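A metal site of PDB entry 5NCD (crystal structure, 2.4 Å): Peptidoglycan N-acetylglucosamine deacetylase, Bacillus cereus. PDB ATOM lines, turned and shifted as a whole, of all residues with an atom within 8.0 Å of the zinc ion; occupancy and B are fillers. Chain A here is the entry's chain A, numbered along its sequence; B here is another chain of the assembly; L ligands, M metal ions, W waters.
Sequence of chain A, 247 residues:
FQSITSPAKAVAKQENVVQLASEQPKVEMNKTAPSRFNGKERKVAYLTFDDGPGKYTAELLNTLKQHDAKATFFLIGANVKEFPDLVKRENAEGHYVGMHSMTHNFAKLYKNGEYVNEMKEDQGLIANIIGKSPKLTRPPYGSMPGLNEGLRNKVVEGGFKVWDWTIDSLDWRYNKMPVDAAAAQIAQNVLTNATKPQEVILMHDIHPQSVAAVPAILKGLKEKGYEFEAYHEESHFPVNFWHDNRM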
ATOM      1  N   PHE A  49      14.998 -23.860  -4.884  1.00  0.00           N
ATOM      2  CA  PHE A  49      14.275 -24.915  -4.196  1.00  0.00           C
ATOM      3  C   PHE A  49      15.178 -25.490  -3.123  1.00  0.00           C
ATOM      4  O   PHE A  49      16.327 -25.825  -3.398  1.00  0.00           O
ATOM      5  CB  PHE A  49      13.849 -26.053  -5.155  1.00  0.00           C
ATOM      6  CG  PHE A  49      13.078 -25.595  -6.365  1.00  0.00           C
ATOM      7  CD1 PHE A  49      11.705 -25.678  -6.393  1.00  0.00           C
ATOM      8  CD2 PHE A  49      13.733 -25.095  -7.472  1.00  0.00           C
ATOM      9  CE1 PHE A  49      10.988 -25.260  -7.510  1.00  0.00           C
ATOM     10  CE2 PHE A  49      13.030 -24.676  -8.591  1.00  0.00           C
ATOM     11  CZ  PHE A  49      11.657 -24.767  -8.613  1.00  0.00           C
ATOM     12  N   ASP A  50      14.629 -25.657  -1.921  1.00  0.00           N
ATOM     13  CA  ASP A  50      15.400 -26.053  -0.762  1.00  0.00           C
ATOM     14  C   ASP A  50      15.111 -27.451  -0.250  1.00  0.00           C
ATOM     15  O   ASP A  50      14.071 -28.011  -0.507  1.00  0.00           O
ATOM     16  CB  ASP A  50      15.134 -25.082   0.397  1.00  0.00           C
ATOM     17  CG  ASP A  50      15.724 -23.701   0.166  1.00  0.00           C
ATOM     18  OD1 ASP A  50      15.943 -23.333  -0.994  1.00  0.00           O
ATOM     19  OD2 ASP A  50      15.948 -22.982   1.167  1.00  0.00           O
ATOM     20  N   ASP A  51      16.037 -27.974   0.526  1.00  0.00           N
ATOM     21  CA  ASP A  51      15.867 -29.155   1.351  1.00  0.00           C
ATOM     22  C   ASP A  51      15.836 -30.423   0.513  1.00  0.00           C
ATOM     23  O   ASP A  51      15.559 -31.507   1.037  1.00  0.00           O
ATOM     24  CB  ASP A  51      14.595 -29.045   2.202  1.00  0.00           C
ATOM     25  CG  ASP A  51      14.426 -27.655   2.859  1.00  0.00           C
ATOM     26  OD1 ASP A  51      15.355 -27.135   3.534  1.00  0.00           O
ATOM     27  OD2 ASP A  51      13.347 -27.068   2.675  1.00  0.00           O
ATOM     28  N   GLY A  52      16.180 -30.304  -0.760  1.00  0.00           N
ATOM     29  CA  GLY A  52      16.190 -31.460  -1.637  1.00  0.00           C
ATOM     30  C   GLY A  52      17.487 -32.230  -1.663  1.00  0.00           C
ATOM     31  O   GLY A  52      18.408 -31.964  -0.878  1.00  0.00           O
ATOM     32  N   PHE A  74      19.156 -25.794  -3.549  1.00  0.00           N
ATOM     33  CA  PHE A  74      20.001 -25.804  -2.374  1.00  0.00           C
ATOM     34  C   PHE A  74      19.735 -27.089  -1.614  1.00  0.00           C
ATOM     35  O   PHE A  74      18.655 -27.306  -1.069  1.00  0.00           O
ATOM     36  CB  PHE A  74      19.744 -24.565  -1.516  1.00  0.00           C
ATOM     37  CG  PHE A  74      20.088 -23.286  -2.209  1.00  0.00           C
ATOM     38  CD1 PHE A  74      21.410 -22.930  -2.378  1.00  0.00           C
ATOM     39  CD2 PHE A  74      19.102 -22.477  -2.721  1.00  0.00           C
ATOM     40  CE1 PHE A  74      21.755 -21.745  -3.031  1.00  0.00           C
ATOM     41  CE2 PHE A  74      19.420 -21.302  -3.366  1.00  0.00           C
ATOM     42  CZ  PHE A  74      20.748 -20.933  -3.535  1.00  0.00           C
ATOM     43  N   ILE A  76      20.262 -30.373   1.004  1.00  0.00           N
ATOM     44  CA  ILE A  76      20.730 -30.809   2.311  1.00  0.00           C
ATOM     45  C   ILE A  76      21.664 -32.010   2.141  1.00  0.00           C
ATOM     46  O   ILE A  76      21.466 -32.863   1.276  1.00  0.00           O
ATOM     47  CB  ILE A  76      19.540 -31.171   3.243  1.00  0.00           C
ATOM     48  CG1 ILE A  76      18.728 -29.914   3.580  1.00  0.00           C
ATOM     49  CG2 ILE A  76      20.027 -31.794   4.541  1.00  0.00           C
ATOM     50  CD1 ILE A  76      17.505 -30.195   4.493  1.00  0.00           C
ATOM     51  N   HIS A 100      22.790 -26.248   1.484  1.00  0.00           N
ATOM     52  CA  HIS A 100      21.711 -25.838   2.367  1.00  0.00           C
ATOM     53  C   HIS A 100      21.948 -26.551   3.697  1.00  0.00           C
ATOM     54  O   HIS A 100      21.027 -26.784   4.457  1.00  0.00           O
ATOM     55  CB  HIS A 100      20.320 -26.157   1.771  1.00  0.00           C
ATOM     56  CG  HIS A 100      19.160 -25.528   2.508  1.00  0.00           C
ATOM     57  ND1 HIS A 100      19.034 -24.170   2.690  1.00  0.00           N
ATOM     58  CD2 HIS A 100      18.059 -26.084   3.076  1.00  0.00           C
ATOM     59  CE1 HIS A 100      17.914 -23.918   3.351  1.00  0.00           C
ATOM     60  NE2 HIS A 100      17.304 -25.072   3.597  1.00  0.00           N
ATOM     61  N   HIS A 104      20.585 -28.873   8.913  1.00  0.00           N
ATOM     62  CA  HIS A 104      19.446 -27.951   8.871  1.00  0.00           C
ATOM     63  C   HIS A 104      18.963 -27.677  10.294  1.00  0.00           C
ATOM     64  O   HIS A 104      17.771 -27.735  10.572  1.00  0.00           O
ATOM     65  CB  HIS A 104      18.308 -28.514   8.026  1.00  0.00           C
ATOM     66  CG  HIS A 104      17.417 -27.489   7.406  1.00  0.00           C
ATOM     67  ND1 HIS A 104      16.422 -26.837   8.096  1.00  0.00           N
ATOM     68  CD2 HIS A 104      17.336 -27.040   6.128  1.00  0.00           C
ATOM     69  CE1 HIS A 104      15.781 -26.011   7.291  1.00  0.00           C
ATOM     70  NE2 HIS A 104      16.297 -26.131   6.086  1.00  0.00           N
ATOM     71  N   ARG A 138      22.744 -21.338   0.837  1.00  0.00           N
ATOM     72  CA  ARG A 138      21.470 -20.763   1.214  1.00  0.00           C
ATOM     73  C   ARG A 138      21.181 -21.217   2.630  1.00  0.00           C
ATOM     74  O   ARG A 138      21.065 -22.432   2.887  1.00  0.00           O
ATOM     75  CB  ARG A 138      20.375 -21.164   0.226  1.00  0.00           C
ATOM     76  CG  ARG A 138      19.000 -21.447   0.790  1.00  0.00           C
ATOM     77  CD  ARG A 138      18.235 -20.180   1.028  1.00  0.00           C
ATOM     78  NE  ARG A 138      18.080 -19.326  -0.148  1.00  0.00           N
ATOM     79  CZ  ARG A 138      17.275 -19.586  -1.172  1.00  0.00           C
ATOM     80  NH1 ARG A 138      16.585 -20.720  -1.202  1.00  0.00           N
ATOM     81  NH2 ARG A 138      17.188 -18.735  -2.187  1.00  0.00           N
ATOM     82  N   PRO A 139      21.141 -20.258   3.562  1.00  0.00           N
ATOM     83  CA  PRO A 139      21.046 -20.526   4.988  1.00  0.00           C
ATOM     84  C   PRO A 139      19.721 -21.161   5.301  1.00  0.00           C
ATOM     85  O   PRO A 139      18.702 -20.677   4.837  1.00  0.00           O
ATOM     86  CB  PRO A 139      21.132 -19.135   5.641  1.00  0.00           C
ATOM     87  CG  PRO A 139      21.450 -18.197   4.583  1.00  0.00           C
ATOM     88  CD  PRO A 139      21.118 -18.810   3.275  1.00  0.00           C
ATOM     89  N   PRO A 140      19.735 -22.241   6.084  1.00  0.00           N
ATOM     90  CA  PRO A 140      18.475 -22.713   6.658  1.00  0.00           C
ATOM     91  C   PRO A 140      17.897 -21.608   7.532  1.00  0.00           C
ATOM     92  O   PRO A 140      18.654 -21.054   8.336  1.00  0.00           O
ATOM     93  CB  PRO A 140      18.890 -23.923   7.491  1.00  0.00           C
ATOM     94  CG  PRO A 140      20.188 -24.353   6.915  1.00  0.00           C
ATOM     95  CD  PRO A 140      20.872 -23.088   6.464  1.00  0.00           C
ATOM     96  N   TYR A 141      16.613 -21.282   7.340  1.00  0.00           N
ATOM     97  CA  TYR A 141      15.880 -20.291   8.125  1.00  0.00           C
ATOM     98  C   TYR A 141      16.253 -18.838   7.819  1.00  0.00           C
ATOM     99  O   TYR A 141      15.913 -17.937   8.591  1.00  0.00           O
ATOM    100  CB  TYR A 141      16.071 -20.546   9.631  1.00  0.00           C
ATOM    101  CG  TYR A 141      15.779 -21.973  10.033  1.00  0.00           C
ATOM    102  CD1 TYR A 141      14.484 -22.473  10.006  1.00  0.00           C
ATOM    103  CD2 TYR A 141      16.785 -22.829  10.456  1.00  0.00           C
ATOM    104  CE1 TYR A 141      14.212 -23.776  10.372  1.00  0.00           C
ATOM    105  CE2 TYR A 141      16.515 -24.132  10.839  1.00  0.00           C
ATOM    106  CZ  TYR A 141      15.225 -24.603  10.800  1.00  0.00           C
ATOM    107  OH  TYR A 141      14.939 -25.907  11.168  1.00  0.00           O
ATOM    108  N   GLY A 142      16.922 -18.619   6.691  1.00  0.00           N
ATOM    109  CA  GLY A 142      17.430 -17.304   6.341  1.00  0.00           C
ATOM    110  C   GLY A 142      18.626 -16.948   7.196  1.00  0.00           C
ATOM    111  O   GLY A 142      18.950 -17.672   8.128  1.00  0.00           O
ATOM    112  N   TRP A 165      16.306 -14.729  -0.094  1.00  0.00           N
ATOM    113  CA  TRP A 165      15.345 -14.630  -1.193  1.00  0.00           C
ATOM    114  C   TRP A 165      14.640 -13.264  -1.228  1.00  0.00           C
ATOM    115  O   TRP A 165      14.776 -12.471  -0.298  1.00  0.00           O
ATOM    116  CB  TRP A 165      14.299 -15.744  -1.086  1.00  0.00           C
ATOM    117  CG  TRP A 165      13.751 -15.814   0.290  1.00  0.00           C
ATOM    118  CD1 TRP A 165      12.655 -15.169   0.758  1.00  0.00           C
ATOM    119  CD2 TRP A 165      14.307 -16.540   1.394  1.00  0.00           C
ATOM    120  NE1 TRP A 165      12.471 -15.459   2.077  1.00  0.00           N
ATOM    121  CE2 TRP A 165      13.470 -16.303   2.501  1.00  0.00           C
ATOM    122  CE3 TRP A 165      15.412 -17.374   1.551  1.00  0.00           C
ATOM    123  CZ2 TRP A 165      13.701 -16.865   3.751  1.00  0.00           C
ATOM    124  CZ3 TRP A 165      15.651 -17.932   2.806  1.00  0.00           C
ATOM    125  CH2 TRP A 165      14.790 -17.675   3.893  1.00  0.00           C
ATOM    126  N   LEU A 202      11.711 -18.372  -3.115  1.00  0.00           N
ATOM    127  CA  LEU A 202      11.947 -19.466  -2.193  1.00  0.00           C
ATOM    128  C   LEU A 202      10.849 -20.494  -2.341  1.00  0.00           C
ATOM    129  O   LEU A 202       9.687 -20.200  -2.071  1.00  0.00           O
ATOM    130  CB  LEU A 202      12.006 -18.957  -0.745  1.00  0.00           C
ATOM    131  CG  LEU A 202      11.982 -20.016   0.356  1.00  0.00           C
ATOM    132  CD1 LEU A 202      13.272 -20.819   0.389  1.00  0.00           C
ATOM    133  CD2 LEU A 202      11.736 -19.390   1.720  1.00  0.00           C
ATOM    134  N   MET A 203      11.210 -21.687  -2.815  1.00  0.00           N
ATOM    135  CA  MET A 203      10.260 -22.789  -2.863  1.00  0.00           C
ATOM    136  C   MET A 203      10.873 -24.036  -2.255  1.00  0.00           C
ATOM    137  O   MET A 203      12.051 -24.016  -1.882  1.00  0.00           O
ATOM    138  CB  MET A 203       9.796 -23.050  -4.296  1.00  0.00           C
ATOM    139  CG  MET A 203       9.095 -21.844  -4.877  1.00  0.00           C
ATOM    140  SD  MET A 203       8.219 -22.212  -6.399  1.00  0.00           S
ATOM    141  CE  MET A 203       6.927 -23.282  -5.784  1.00  0.00           C
ATOM    142  N   HIS A 204      10.086 -25.093  -2.106  1.00  0.00           N
ATOM    143  CA  HIS A 204      10.589 -26.339  -1.532  1.00  0.00           C
ATOM    144  C   HIS A 204      10.141 -27.548  -2.378  1.00  0.00           C
ATOM    145  O   HIS A 204       8.968 -27.836  -2.469  1.00  0.00           O
ATOM    146  CB  HIS A 204      10.108 -26.473  -0.082  1.00  0.00           C
ATOM    147  CG  HIS A 204      10.517 -25.322   0.791  1.00  0.00           C
ATOM    148  ND1 HIS A 204      10.061 -24.041   0.596  1.00  0.00           N
ATOM    149  CD2 HIS A 204      11.335 -25.267   1.871  1.00  0.00           C
ATOM    150  CE1 HIS A 204      10.600 -23.246   1.500  1.00  0.00           C
ATOM    151  NE2 HIS A 204      11.377 -23.961   2.284  1.00  0.00           N
ATOM    152  N   ILE A 206      10.586 -30.682  -1.894  1.00  0.00           N
ATOM    153  CA  ILE A 206      10.220 -31.841  -1.094  1.00  0.00           C
ATOM    154  C   ILE A 206       8.710 -31.885  -0.851  1.00  0.00           C
ATOM    155  O   ILE A 206       8.202 -32.862  -0.331  1.00  0.00           O
ATOM    156  CB  ILE A 206      10.934 -31.836   0.264  1.00  0.00           C
ATOM    157  CG1 ILE A 206      10.787 -30.457   0.936  1.00  0.00           C
ATOM    158  CG2 ILE A 206      12.406 -32.185   0.076  1.00  0.00           C
ATOM    159  CD1 ILE A 206      10.747 -30.491   2.479  1.00  0.00           C
ATOM    160  N   HIS B 243       7.919 -23.518  10.495  1.00  0.00           N
ATOM    161  CA  HIS B 243       7.063 -23.775   9.325  1.00  0.00           C
ATOM    162  C   HIS B 243       6.109 -24.936   9.613  1.00  0.00           C
ATOM    163  O   HIS B 243       5.822 -25.752   8.729  1.00  0.00           O
ATOM    164  CB  HIS B 243       7.885 -24.084   8.063  1.00  0.00           C
ATOM    165  CG  HIS B 243       9.046 -23.165   7.832  1.00  0.00           C
ATOM    166  ND1 HIS B 243       9.041 -21.837   8.216  1.00  0.00           N
ATOM    167  CD2 HIS B 243      10.260 -23.389   7.266  1.00  0.00           C
ATOM    168  CE1 HIS B 243      10.196 -21.281   7.886  1.00  0.00           C
ATOM    169  NE2 HIS B 243      10.950 -22.207   7.314  1.00  0.00           N
HETATM  170  C1  LIG L   1      14.313 -22.697   4.601  1.00  0.00           C
HETATM  171  O1  LIG L   1      14.551 -23.297   3.504  1.00  0.00           O
HETATM  172  O2  LIG L   1      15.026 -22.983   5.591  1.00  0.00           O
HETATM  173  C2  LIG L   1      13.228 -21.656   4.773  1.00  0.00           C
HETATM  174 ZN    ZN M   1      15.313 -25.175   4.570  1.00  0.00          ZN
HETATM  175  O   HOH W   1      12.475 -25.117   5.733  1.00  0.00           O
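The zinc ion is bound by NE2 of His 104, OD1 of Asp 51, NE2 of His 100, O1 of the ligand and O2 of the ligand. The zinc ion has five donor atoms within binding distance.
Three residues have an atom within 4 Å of the zinc ion: Asp 51, His 100 and His 104.
The backbone carbonyl oxygen (O) of Phe 74 sits at hydrogen-bond distance from the backbone NH (N) of Asp 51. NE2 of His 100 sits close to OD2 of Asp 50, at 3.5 Å. O of His 104 is in hydrogen-bond range of OH of Tyr 141 (3.4 Å). ND1 of His 100 sits at hydrogen-bond distance from O of Arg 138 (2.7 Å).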
